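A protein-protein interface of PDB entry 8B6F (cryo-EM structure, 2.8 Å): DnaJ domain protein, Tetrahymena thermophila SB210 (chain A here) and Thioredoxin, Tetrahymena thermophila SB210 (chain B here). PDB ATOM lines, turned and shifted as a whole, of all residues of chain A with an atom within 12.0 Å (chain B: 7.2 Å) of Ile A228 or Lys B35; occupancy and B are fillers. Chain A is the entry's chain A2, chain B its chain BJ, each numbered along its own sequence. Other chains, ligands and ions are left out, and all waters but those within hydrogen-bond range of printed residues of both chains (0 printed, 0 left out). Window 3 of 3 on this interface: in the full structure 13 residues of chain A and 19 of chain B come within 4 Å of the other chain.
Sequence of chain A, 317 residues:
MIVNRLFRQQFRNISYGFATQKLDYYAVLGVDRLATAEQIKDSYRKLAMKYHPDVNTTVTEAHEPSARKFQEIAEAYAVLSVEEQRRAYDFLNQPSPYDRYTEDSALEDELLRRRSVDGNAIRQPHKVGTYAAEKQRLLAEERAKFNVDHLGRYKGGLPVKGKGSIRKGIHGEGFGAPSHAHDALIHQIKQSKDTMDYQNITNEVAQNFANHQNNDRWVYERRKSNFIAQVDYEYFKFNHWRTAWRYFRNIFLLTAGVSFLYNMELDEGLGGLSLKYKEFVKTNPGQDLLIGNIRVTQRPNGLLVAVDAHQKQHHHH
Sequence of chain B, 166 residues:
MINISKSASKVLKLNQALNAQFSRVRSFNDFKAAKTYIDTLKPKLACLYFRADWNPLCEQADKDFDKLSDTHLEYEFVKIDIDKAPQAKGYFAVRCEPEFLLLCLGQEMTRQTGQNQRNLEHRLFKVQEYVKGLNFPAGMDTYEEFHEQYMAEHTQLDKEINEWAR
Of the 22 printed residues of chain B, 4 touch a printed residue of chain A.
Of the 9 printed residues of chain A, 3 touch a printed residue of chain B.
Of the printed residues of chain B, Ser A225 touches Tyr B91 and His B147.
Printed residues of chain B within 4 Å of Asn A226: Tyr B91.
Ile A228 touches just these residues of chain B: Phe B31 (3.8 Å), Lys B35 (3.7 Å) and Tyr B91 (3.5 Å).
Lys B35 touches just one residue of chain A: Ile A228 (3.7 Å).
Thr B36 touches none of the printed residues of chain A.
Ile B38 touches none of the printed residues of chain A.
No residue of chain A comes within 4 Å of Asp B39.
Tyr B91 touches three residues of chain A.
Printed residues of chain A within 4 Å of His B147: Ser A225.
The nearest residue of chain B that does not touch Ile A228 is Glu B145 (5.8 Å).
The nearest residue of chain A that does not touch Lys B35 is Asn A226 (8.0 Å).
NZ of Lys B35 is in salt-bridge range of OD2 of Asp B39, at 3.4 Å.
NZ of Lys B35 lies within hydrogen-bond range of OH of Tyr B91, at 2.7 Å.
The side-chain amino group (NZ) of Lys B35 lies within salt-bridge range of the side-chain carboxylate (OE1) of Glu B145 (2.6 Å).
OH of Tyr B91 lies within hydrogen-bond range of ND1 of His B147 (3.1 Å).
The side-chain carboxylate (OE1) of Glu B145 sits close to a ring nitrogen (ND1) of His B147.
Tyr B91 touches Ser A225.
CB of His B147 touches OG of Ser A225, at 3.4 Å.
O of Asn A226 touches CD1 of Tyr B91, 3.8 Å away.
CZ of Phe B31 touches CD1 of Ile A228, 3.8 Å away.
Ile A228 touches Lys B35 (CD1 to CE, 3.7 Å).
Tyr B91 touches Ile A228.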
ATOM      1  N   LYS A 224     -34.912  -3.399 -26.839  1.00  0.00           N
ATOM      2  CA  LYS A 224     -33.989  -3.660 -25.745  1.00  0.00           C
ATOM      3  C   LYS A 224     -32.613  -3.982 -26.312  1.00  0.00           C
ATOM      4  O   LYS A 224     -32.488  -4.823 -27.206  1.00  0.00           O
ATOM      5  CB  LYS A 224     -34.492  -4.815 -24.877  1.00  0.00           C
ATOM      6  CG  LYS A 224     -35.935  -4.644 -24.413  1.00  0.00           C
ATOM      7  CD  LYS A 224     -36.350  -5.730 -23.430  1.00  0.00           C
ATOM      8  CE  LYS A 224     -36.444  -7.094 -24.093  1.00  0.00           C
ATOM      9  NZ  LYS A 224     -37.450  -7.119 -25.193  1.00  0.00           N
ATOM     10  N   SER A 225     -31.588  -3.321 -25.784  1.00  0.00           N
ATOM     11  CA  SER A 225     -30.221  -3.471 -26.262  1.00  0.00           C
ATOM     12  C   SER A 225     -29.450  -4.401 -25.337  1.00  0.00           C
ATOM     13  O   SER A 225     -29.501  -4.249 -24.113  1.00  0.00           O
ATOM     14  CB  SER A 225     -29.523  -2.112 -26.344  1.00  0.00           C
ATOM     15  OG  SER A 225     -29.559  -1.446 -25.096  1.00  0.00           O
ATOM     16  N   ASN A 226     -28.734  -5.356 -25.925  1.00  0.00           N
ATOM     17  CA  ASN A 226     -27.937  -6.282 -25.133  1.00  0.00           C
ATOM     18  C   ASN A 226     -26.843  -5.535 -24.382  1.00  0.00           C
ATOM     19  O   ASN A 226     -26.299  -4.536 -24.857  1.00  0.00           O
ATOM     20  CB  ASN A 226     -27.312  -7.351 -26.029  1.00  0.00           C
ATOM     21  CG  ASN A 226     -28.341  -8.284 -26.627  1.00  0.00           C
ATOM     22  OD1 ASN A 226     -29.535  -7.989 -26.631  1.00  0.00           O
ATOM     23  ND2 ASN A 226     -27.882  -9.419 -27.139  1.00  0.00           N
ATOM     24  N   PHE A 227     -26.522  -6.035 -23.193  1.00  0.00           N
ATOM     25  CA  PHE A 227     -25.520  -5.395 -22.358  1.00  0.00           C
ATOM     26  C   PHE A 227     -24.120  -5.631 -22.912  1.00  0.00           C
ATOM     27  O   PHE A 227     -23.845  -6.639 -23.568  1.00  0.00           O
ATOM     28  CB  PHE A 227     -25.599  -5.924 -20.927  1.00  0.00           C
ATOM     29  CG  PHE A 227     -26.988  -5.937 -20.360  1.00  0.00           C
ATOM     30  CD1 PHE A 227     -27.545  -4.788 -19.826  1.00  0.00           C
ATOM     31  CD2 PHE A 227     -27.733  -7.106 -20.349  1.00  0.00           C
ATOM     32  CE1 PHE A 227     -28.821  -4.800 -19.299  1.00  0.00           C
ATOM     33  CE2 PHE A 227     -29.008  -7.124 -19.825  1.00  0.00           C
ATOM     34  CZ  PHE A 227     -29.553  -5.969 -19.299  1.00  0.00           C
ATOM     35  N   ILE A 228     -23.229  -4.681 -22.641  1.00  0.00           N
ATOM     36  CA  ILE A 228     -21.804  -4.810 -22.924  1.00  0.00           C
ATOM     37  C   ILE A 228     -21.072  -4.844 -21.592  1.00  0.00           C
ATOM     38  O   ILE A 228     -21.235  -3.940 -20.764  1.00  0.00           O
ATOM     39  CB  ILE A 228     -21.289  -3.659 -23.805  1.00  0.00           C
ATOM     40  CG1 ILE A 228     -21.975  -3.691 -25.173  1.00  0.00           C
ATOM     41  CG2 ILE A 228     -19.773  -3.748 -23.968  1.00  0.00           C
ATOM     42  CD1 ILE A 228     -21.670  -2.492 -26.045  1.00  0.00           C
ATOM     43  N   ALA A 229     -20.271  -5.884 -21.387  1.00  0.00           N
ATOM     44  CA  ALA A 229     -19.584  -6.091 -20.122  1.00  0.00           C
ATOM     45  C   ALA A 229     -18.201  -5.458 -20.169  1.00  0.00           C
ATOM     46  O   ALA A 229     -17.432  -5.695 -21.106  1.00  0.00           O
ATOM     47  CB  ALA A 229     -19.473  -7.583 -19.809  1.00  0.00           C
ATOM     48  N   GLN A 230     -17.892  -4.651 -19.159  1.00  0.00           N
ATOM     49  CA  GLN A 230     -16.579  -4.048 -19.001  1.00  0.00           C
ATOM     50  C   GLN A 230     -16.127  -4.218 -17.559  1.00  0.00           C
ATOM     51  O   GLN A 230     -16.947  -4.347 -16.647  1.00  0.00           O
ATOM     52  CB  GLN A 230     -16.586  -2.557 -19.372  1.00  0.00           C
ATOM     53  CG  GLN A 230     -17.472  -1.698 -18.484  1.00  0.00           C
ATOM     54  CD  GLN A 230     -17.332  -0.219 -18.777  1.00  0.00           C
ATOM     55  OE1 GLN A 230     -16.768   0.172 -19.797  1.00  0.00           O
ATOM     56  NE2 GLN A 230     -17.842   0.613 -17.878  1.00  0.00           N
ATOM     57  N   VAL A 231     -14.815  -4.221 -17.363  1.00  0.00           N
ATOM     58  CA  VAL A 231     -14.244  -4.365 -16.029  1.00  0.00           C
ATOM     59  C   VAL A 231     -14.269  -3.012 -15.334  1.00  0.00           C
ATOM     60  O   VAL A 231     -13.843  -2.000 -15.903  1.00  0.00           O
ATOM     61  CB  VAL A 231     -12.816  -4.928 -16.105  1.00  0.00           C
ATOM     62  CG1 VAL A 231     -12.262  -5.162 -14.710  1.00  0.00           C
ATOM     63  CG2 VAL A 231     -12.795  -6.214 -16.914  1.00  0.00           C
ATOM     64  N   ASP A 232     -14.777  -2.989 -14.104  1.00  0.00           N
ATOM     65  CA  ASP A 232     -14.862  -1.773 -13.303  1.00  0.00           C
ATOM     66  C   ASP A 232     -13.661  -1.739 -12.365  1.00  0.00           C
ATOM     67  O   ASP A 232     -13.568  -2.547 -11.436  1.00  0.00           O
ATOM     68  CB  ASP A 232     -16.173  -1.733 -12.522  1.00  0.00           C
ATOM     69  CG  ASP A 232     -16.446  -0.377 -11.907  1.00  0.00           C
ATOM     70  OD1 ASP A 232     -15.478   0.320 -11.543  1.00  0.00           O
ATOM     71  OD2 ASP A 232     -17.631  -0.006 -11.788  1.00  0.00           O
ATOM     72  N   PHE B  28     -19.006  -1.653 -42.116  1.00  0.00           N
ATOM     73  CA  PHE B  28     -18.270  -2.281 -41.031  1.00  0.00           C
ATOM     74  C   PHE B  28     -18.642  -3.752 -40.947  1.00  0.00           C
ATOM     75  O   PHE B  28     -19.796  -4.126 -41.177  1.00  0.00           O
ATOM     76  CB  PHE B  28     -18.560  -1.602 -39.689  1.00  0.00           C
ATOM     77  CG  PHE B  28     -18.102  -0.176 -39.620  1.00  0.00           C
ATOM     78  CD1 PHE B  28     -16.804   0.128 -39.248  1.00  0.00           C
ATOM     79  CD2 PHE B  28     -18.969   0.859 -39.920  1.00  0.00           C
ATOM     80  CE1 PHE B  28     -16.378   1.438 -39.179  1.00  0.00           C
ATOM     81  CE2 PHE B  28     -18.550   2.173 -39.854  1.00  0.00           C
ATOM     82  CZ  PHE B  28     -17.252   2.461 -39.482  1.00  0.00           C
ATOM     83  N   ASP B  30     -17.130  -5.471 -38.082  1.00  0.00           N
ATOM     84  CA  ASP B  30     -16.888  -5.716 -36.668  1.00  0.00           C
ATOM     85  C   ASP B  30     -17.766  -4.792 -35.836  1.00  0.00           C
ATOM     86  O   ASP B  30     -17.778  -3.577 -36.055  1.00  0.00           O
ATOM     87  CB  ASP B  30     -15.414  -5.494 -36.324  1.00  0.00           C
ATOM     88  CG  ASP B  30     -15.093  -5.844 -34.884  1.00  0.00           C
ATOM     89  OD1 ASP B  30     -15.979  -6.385 -34.191  1.00  0.00           O
ATOM     90  OD2 ASP B  30     -13.957  -5.575 -34.444  1.00  0.00           O
ATOM     91  N   PHE B  31     -18.500  -5.374 -34.887  1.00  0.00           N
ATOM     92  CA  PHE B  31     -19.377  -4.576 -34.038  1.00  0.00           C
ATOM     93  C   PHE B  31     -18.583  -3.571 -33.215  1.00  0.00           C
ATOM     94  O   PHE B  31     -18.992  -2.414 -33.074  1.00  0.00           O
ATOM     95  CB  PHE B  31     -20.193  -5.488 -33.124  1.00  0.00           C
ATOM     96  CG  PHE B  31     -20.748  -4.794 -31.916  1.00  0.00           C
ATOM     97  CD1 PHE B  31     -21.859  -3.976 -32.022  1.00  0.00           C
ATOM     98  CD2 PHE B  31     -20.161  -4.965 -30.673  1.00  0.00           C
ATOM     99  CE1 PHE B  31     -22.374  -3.338 -30.910  1.00  0.00           C
ATOM    100  CE2 PHE B  31     -20.670  -4.328 -29.559  1.00  0.00           C
ATOM    101  CZ  PHE B  31     -21.777  -3.514 -29.678  1.00  0.00           C
ATOM    102  N   LYS B  32     -17.444  -3.994 -32.664  1.00  0.00           N
ATOM    103  CA  LYS B  32     -16.625  -3.081 -31.876  1.00  0.00           C
ATOM    104  C   LYS B  32     -16.168  -1.899 -32.720  1.00  0.00           C
ATOM    105  O   LYS B  32     -16.250  -0.744 -32.288  1.00  0.00           O
ATOM    106  CB  LYS B  32     -15.426  -3.830 -31.293  1.00  0.00           C
ATOM    107  CG  LYS B  32     -14.400  -2.942 -30.590  1.00  0.00           C
ATOM    108  CD  LYS B  32     -15.003  -2.159 -29.431  1.00  0.00           C
ATOM    109  CE  LYS B  32     -15.445  -3.067 -28.293  1.00  0.00           C
ATOM    110  NZ  LYS B  32     -14.316  -3.864 -27.736  1.00  0.00           N
ATOM    111  N   ALA B  33     -15.678  -2.171 -33.929  1.00  0.00           N
ATOM    112  CA  ALA B  33     -15.217  -1.092 -34.794  1.00  0.00           C
ATOM    113  C   ALA B  33     -16.358  -0.152 -35.161  1.00  0.00           C
ATOM    114  O   ALA B  33     -16.200   1.073 -35.126  1.00  0.00           O
ATOM    115  CB  ALA B  33     -14.574  -1.670 -36.053  1.00  0.00           C
ATOM    116  N   ALA B  34     -17.517  -0.707 -35.519  1.00  0.00           N
ATOM    117  CA  ALA B  34     -18.648   0.130 -35.907  1.00  0.00           C
ATOM    118  C   ALA B  34     -19.095   1.015 -34.751  1.00  0.00           C
ATOM    119  O   ALA B  34     -19.321   2.217 -34.924  1.00  0.00           O
ATOM    120  CB  ALA B  34     -19.803  -0.744 -36.392  1.00  0.00           C
ATOM    121  N   LYS B  35     -19.235   0.433 -33.559  1.00  0.00           N
ATOM    122  CA  LYS B  35     -19.674   1.212 -32.407  1.00  0.00           C
ATOM    123  C   LYS B  35     -18.655   2.284 -32.047  1.00  0.00           C
ATOM    124  O   LYS B  35     -19.026   3.419 -31.727  1.00  0.00           O
ATOM    125  CB  LYS B  35     -19.929   0.289 -31.215  1.00  0.00           C
ATOM    126  CG  LYS B  35     -20.336   1.026 -29.949  1.00  0.00           C
ATOM    127  CD  LYS B  35     -20.779   0.061 -28.864  1.00  0.00           C
ATOM    128  CE  LYS B  35     -21.041   0.788 -27.557  1.00  0.00           C
ATOM    129  NZ  LYS B  35     -22.018   1.896 -27.715  1.00  0.00           N
ATOM    130  N   THR B  36     -17.366   1.944 -32.089  1.00  0.00           N
ATOM    131  CA  THR B  36     -16.337   2.931 -31.780  1.00  0.00           C
ATOM    132  C   THR B  36     -16.365   4.081 -32.778  1.00  0.00           C
ATOM    133  O   THR B  36     -16.256   5.250 -32.392  1.00  0.00           O
ATOM    134  CB  THR B  36     -14.960   2.269 -31.770  1.00  0.00           C
ATOM    135  OG1 THR B  36     -14.943   1.204 -30.811  1.00  0.00           O
ATOM    136  CG2 THR B  36     -13.875   3.279 -31.413  1.00  0.00           C
ATOM    137  N   TYR B  37     -16.506   3.770 -34.067  1.00  0.00           N
ATOM    138  CA  TYR B  37     -16.561   4.823 -35.076  1.00  0.00           C
ATOM    139  C   TYR B  37     -17.757   5.738 -34.847  1.00  0.00           C
ATOM    140  O   TYR B  37     -17.630   6.967 -34.889  1.00  0.00           O
ATOM    141  CB  TYR B  37     -16.621   4.200 -36.469  1.00  0.00           C
ATOM    142  CG  TYR B  37     -16.989   5.177 -37.560  1.00  0.00           C
ATOM    143  CD1 TYR B  37     -16.027   5.981 -38.155  1.00  0.00           C
ATOM    144  CD2 TYR B  37     -18.300   5.286 -38.001  1.00  0.00           C
ATOM    145  CE1 TYR B  37     -16.363   6.872 -39.155  1.00  0.00           C
ATOM    146  CE2 TYR B  37     -18.646   6.172 -38.999  1.00  0.00           C
ATOM    147  CZ  TYR B  37     -17.673   6.962 -39.573  1.00  0.00           C
ATOM    148  OH  TYR B  37     -18.017   7.846 -40.567  1.00  0.00           O
ATOM    149  N   ILE B  38     -18.932   5.156 -34.605  1.00  0.00           N
ATOM    150  CA  ILE B  38     -20.128   5.970 -34.409  1.00  0.00           C
ATOM    151  C   ILE B  38     -19.977   6.837 -33.168  1.00  0.00           C
ATOM    152  O   ILE B  38     -20.301   8.030 -33.182  1.00  0.00           O
ATOM    153  CB  ILE B  38     -21.379   5.073 -34.332  1.00  0.00           C
ATOM    154  CG1 ILE B  38     -21.572   4.317 -35.648  1.00  0.00           C
ATOM    155  CG2 ILE B  38     -22.619   5.907 -34.033  1.00  0.00           C
ATOM    156  CD1 ILE B  38     -22.622   3.226 -35.586  1.00  0.00           C
ATOM    157  N   ASP B  39     -19.487   6.253 -32.073  1.00  0.00           N
ATOM    158  CA  ASP B  39     -19.326   7.017 -30.841  1.00  0.00           C
ATOM    159  C   ASP B  39     -18.331   8.153 -31.022  1.00  0.00           C
ATOM    160  O   ASP B  39     -18.555   9.267 -30.536  1.00  0.00           O
ATOM    161  CB  ASP B  39     -18.879   6.098 -29.705  1.00  0.00           C
ATOM    162  CG  ASP B  39     -19.924   5.059 -29.350  1.00  0.00           C
ATOM    163  OD1 ASP B  39     -21.011   5.072 -29.961  1.00  0.00           O
ATOM    164  OD2 ASP B  39     -19.656   4.230 -28.457  1.00  0.00           O
ATOM    165  N   THR B  40     -17.215   7.889 -31.705  1.00  0.00           N
ATOM    166  CA  THR B  40     -16.228   8.938 -31.932  1.00  0.00           C
ATOM    167  C   THR B  40     -16.795  10.052 -32.800  1.00  0.00           C
ATOM    168  O   THR B  40     -16.576  11.238 -32.526  1.00  0.00           O
ATOM    169  CB  THR B  40     -14.973   8.344 -32.575  1.00  0.00           C
ATOM    170  OG1 THR B  40     -14.411   7.350 -31.709  1.00  0.00           O
ATOM    171  CG2 THR B  40     -13.932   9.425 -32.839  1.00  0.00           C
ATOM    172  N   LEU B  41     -17.525   9.691 -33.856  1.00  0.00           N
ATOM    173  CA  LEU B  41     -18.062  10.701 -34.762  1.00  0.00           C
ATOM    174  C   LEU B  41     -19.127  11.554 -34.083  1.00  0.00           C
ATOM    175  O   LEU B  41     -19.190  12.769 -34.307  1.00  0.00           O
ATOM    176  CB  LEU B  41     -18.621  10.028 -36.013  1.00  0.00           C
ATOM    177  CG  LEU B  41     -19.223  10.953 -37.070  1.00  0.00           C
ATOM    178  CD1 LEU B  41     -18.263  12.066 -37.454  1.00  0.00           C
ATOM    179  CD2 LEU B  41     -19.599  10.142 -38.285  1.00  0.00           C
ATOM    180  N   VAL B  78     -24.238   4.518 -42.130  1.00  0.00           N
ATOM    181  CA  VAL B  78     -23.391   3.428 -41.666  1.00  0.00           C
ATOM    182  C   VAL B  78     -24.060   2.113 -42.032  1.00  0.00           C
ATOM    183  O   VAL B  78     -25.286   1.981 -41.943  1.00  0.00           O
ATOM    184  CB  VAL B  78     -23.134   3.506 -40.147  1.00  0.00           C
ATOM    185  CG1 VAL B  78     -22.258   2.352 -39.690  1.00  0.00           C
ATOM    186  CG2 VAL B  78     -22.495   4.835 -39.787  1.00  0.00           C
ATOM    187  N   ILE B  80     -23.859  -2.184 -41.560  1.00  0.00           N
ATOM    188  CA  ILE B  80     -23.367  -3.269 -40.720  1.00  0.00           C
ATOM    189  C   ILE B  80     -23.949  -4.576 -41.236  1.00  0.00           C
ATOM    190  O   ILE B  80     -25.150  -4.661 -41.512  1.00  0.00           O
ATOM    191  CB  ILE B  80     -23.736  -3.063 -39.238  1.00  0.00           C
ATOM    192  CG1 ILE B  80     -23.194  -1.716 -38.748  1.00  0.00           C
ATOM    193  CG2 ILE B  80     -23.196  -4.214 -38.393  1.00  0.00           C
ATOM    194  CD1 ILE B  80     -23.476  -1.413 -37.287  1.00  0.00           C
ATOM    195  N   GLN B  87     -22.834  -9.418 -32.623  1.00  0.00           N
ATOM    196  CA  GLN B  87     -23.197  -8.614 -31.460  1.00  0.00           C
ATOM    197  C   GLN B  87     -24.032  -7.404 -31.853  1.00  0.00           C
ATOM    198  O   GLN B  87     -24.800  -6.891 -31.031  1.00  0.00           O
ATOM    199  CB  GLN B  87     -21.945  -8.154 -30.711  1.00  0.00           C
ATOM    200  CG  GLN B  87     -20.989  -9.268 -30.332  1.00  0.00           C
ATOM    201  CD  GLN B  87     -19.907  -9.483 -31.369  1.00  0.00           C
ATOM    202  OE1 GLN B  87     -20.113  -9.239 -32.557  1.00  0.00           O
ATOM    203  NE2 GLN B  87     -18.741  -9.930 -30.922  1.00  0.00           N
ATOM    204  N   TYR B  91     -27.200  -5.710 -29.804  1.00  0.00           N
ATOM    205  CA  TYR B  91     -27.007  -4.371 -29.259  1.00  0.00           C
ATOM    206  C   TYR B  91     -28.044  -3.393 -29.794  1.00  0.00           C
ATOM    207  O   TYR B  91     -28.580  -2.573 -29.039  1.00  0.00           O
ATOM    208  CB  TYR B  91     -25.599  -3.869 -29.573  1.00  0.00           C
ATOM    209  CG  TYR B  91     -25.321  -2.507 -28.983  1.00  0.00           C
ATOM    210  CD1 TYR B  91     -24.937  -2.370 -27.657  1.00  0.00           C
ATOM    211  CD2 TYR B  91     -25.458  -1.359 -29.749  1.00  0.00           C
ATOM    212  CE1 TYR B  91     -24.692  -1.127 -27.111  1.00  0.00           C
ATOM    213  CE2 TYR B  91     -25.215  -0.111 -29.211  1.00  0.00           C
ATOM    214  CZ  TYR B  91     -24.834  -0.003 -27.892  1.00  0.00           C
ATOM    215  OH  TYR B  91     -24.589   1.237 -27.355  1.00  0.00           O
ATOM    216  N   PHE B  92     -28.337  -3.454 -31.089  1.00  0.00           N
ATOM    217  CA  PHE B  92     -29.275  -2.533 -31.715  1.00  0.00           C
ATOM    218  C   PHE B  92     -30.697  -3.073 -31.755  1.00  0.00           C
ATOM    219  O   PHE B  92     -31.568  -2.445 -32.363  1.00  0.00           O
ATOM    220  CB  PHE B  92     -28.808  -2.189 -33.132  1.00  0.00           C
ATOM    221  CG  PHE B  92     -27.560  -1.361 -33.168  1.00  0.00           C
ATOM    222  CD1 PHE B  92     -27.613   0.001 -32.930  1.00  0.00           C
ATOM    223  CD2 PHE B  92     -26.333  -1.941 -33.439  1.00  0.00           C
ATOM    224  CE1 PHE B  92     -26.468   0.769 -32.959  1.00  0.00           C
ATOM    225  CE2 PHE B  92     -25.182  -1.176 -33.469  1.00  0.00           C
ATOM    226  CZ  PHE B  92     -25.251   0.180 -33.230  1.00  0.00           C
ATOM    227  N   TYR B 143     -24.308  14.114 -27.778  1.00  0.00           N
ATOM    228  CA  TYR B 143     -24.550  12.778 -28.300  1.00  0.00           C
ATOM    229  C   TYR B 143     -24.543  11.754 -27.171  1.00  0.00           C
ATOM    230  O   TYR B 143     -23.788  11.873 -26.204  1.00  0.00           O
ATOM    231  CB  TYR B 143     -23.487  12.429 -29.342  1.00  0.00           C
ATOM    232  CG  TYR B 143     -23.547  11.007 -29.843  1.00  0.00           C
ATOM    233  CD1 TYR B 143     -22.826  10.002 -29.216  1.00  0.00           C
ATOM    234  CD2 TYR B 143     -24.311  10.673 -30.951  1.00  0.00           C
ATOM    235  CE1 TYR B 143     -22.871   8.703 -29.671  1.00  0.00           C
ATOM    236  CE2 TYR B 143     -24.363   9.376 -31.415  1.00  0.00           C
ATOM    237  CZ  TYR B 143     -23.642   8.396 -30.769  1.00  0.00           C
ATOM    238  OH  TYR B 143     -23.687   7.101 -31.224  1.00  0.00           O
ATOM    239  N   GLU B 145     -24.902   7.314 -26.402  1.00  0.00           N
ATOM    240  CA  GLU B 145     -24.871   5.986 -26.992  1.00  0.00           C
ATOM    241  C   GLU B 145     -26.282   5.408 -27.065  1.00  0.00           C
ATOM    242  O   GLU B 145     -27.194   5.824 -26.347  1.00  0.00           O
ATOM    243  CB  GLU B 145     -23.956   5.061 -26.192  1.00  0.00           C
ATOM    244  CG  GLU B 145     -22.500   5.506 -26.196  1.00  0.00           C
ATOM    245  CD  GLU B 145     -21.564   4.460 -25.623  1.00  0.00           C
ATOM    246  OE1 GLU B 145     -21.970   3.285 -25.521  1.00  0.00           O
ATOM    247  OE2 GLU B 145     -20.418   4.815 -25.275  1.00  0.00           O
ATOM    248  N   PHE B 146     -26.453   4.431 -27.958  1.00  0.00           N
ATOM    249  CA  PHE B 146     -27.788   3.918 -28.245  1.00  0.00           C
ATOM    250  C   PHE B 146     -28.439   3.327 -27.001  1.00  0.00           C
ATOM    251  O   PHE B 146     -29.655   3.447 -26.813  1.00  0.00           O
ATOM    252  CB  PHE B 146     -27.716   2.871 -29.356  1.00  0.00           C
ATOM    253  CG  PHE B 146     -29.044   2.267 -29.698  1.00  0.00           C
ATOM    254  CD1 PHE B 146     -29.928   2.933 -30.527  1.00  0.00           C
ATOM    255  CD2 PHE B 146     -29.406   1.029 -29.196  1.00  0.00           C
ATOM    256  CE1 PHE B 146     -31.150   2.381 -30.845  1.00  0.00           C
ATOM    257  CE2 PHE B 146     -30.627   0.470 -29.511  1.00  0.00           C
ATOM    258  CZ  PHE B 146     -31.501   1.148 -30.337  1.00  0.00           C
ATOM    259  N   HIS B 147     -27.651   2.684 -26.143  1.00  0.00           N
ATOM    260  CA  HIS B 147     -28.194   1.960 -25.001  1.00  0.00           C
ATOM    261  C   HIS B 147     -28.517   2.854 -23.812  1.00  0.00           C
ATOM    262  O   HIS B 147     -29.135   2.377 -22.856  1.00  0.00           O
ATOM    263  CB  HIS B 147     -27.205   0.883 -24.551  1.00  0.00           C
ATOM    264  CG  HIS B 147     -26.031   1.427 -23.800  1.00  0.00           C
ATOM    265  ND1 HIS B 147     -24.968   2.045 -24.422  1.00  0.00           N
ATOM    266  CD2 HIS B 147     -25.756   1.454 -22.474  1.00  0.00           C
ATOM    267  CE1 HIS B 147     -24.088   2.425 -23.514  1.00  0.00           C
ATOM    268  NE2 HIS B 147     -24.542   2.079 -22.323  1.00  0.00           N
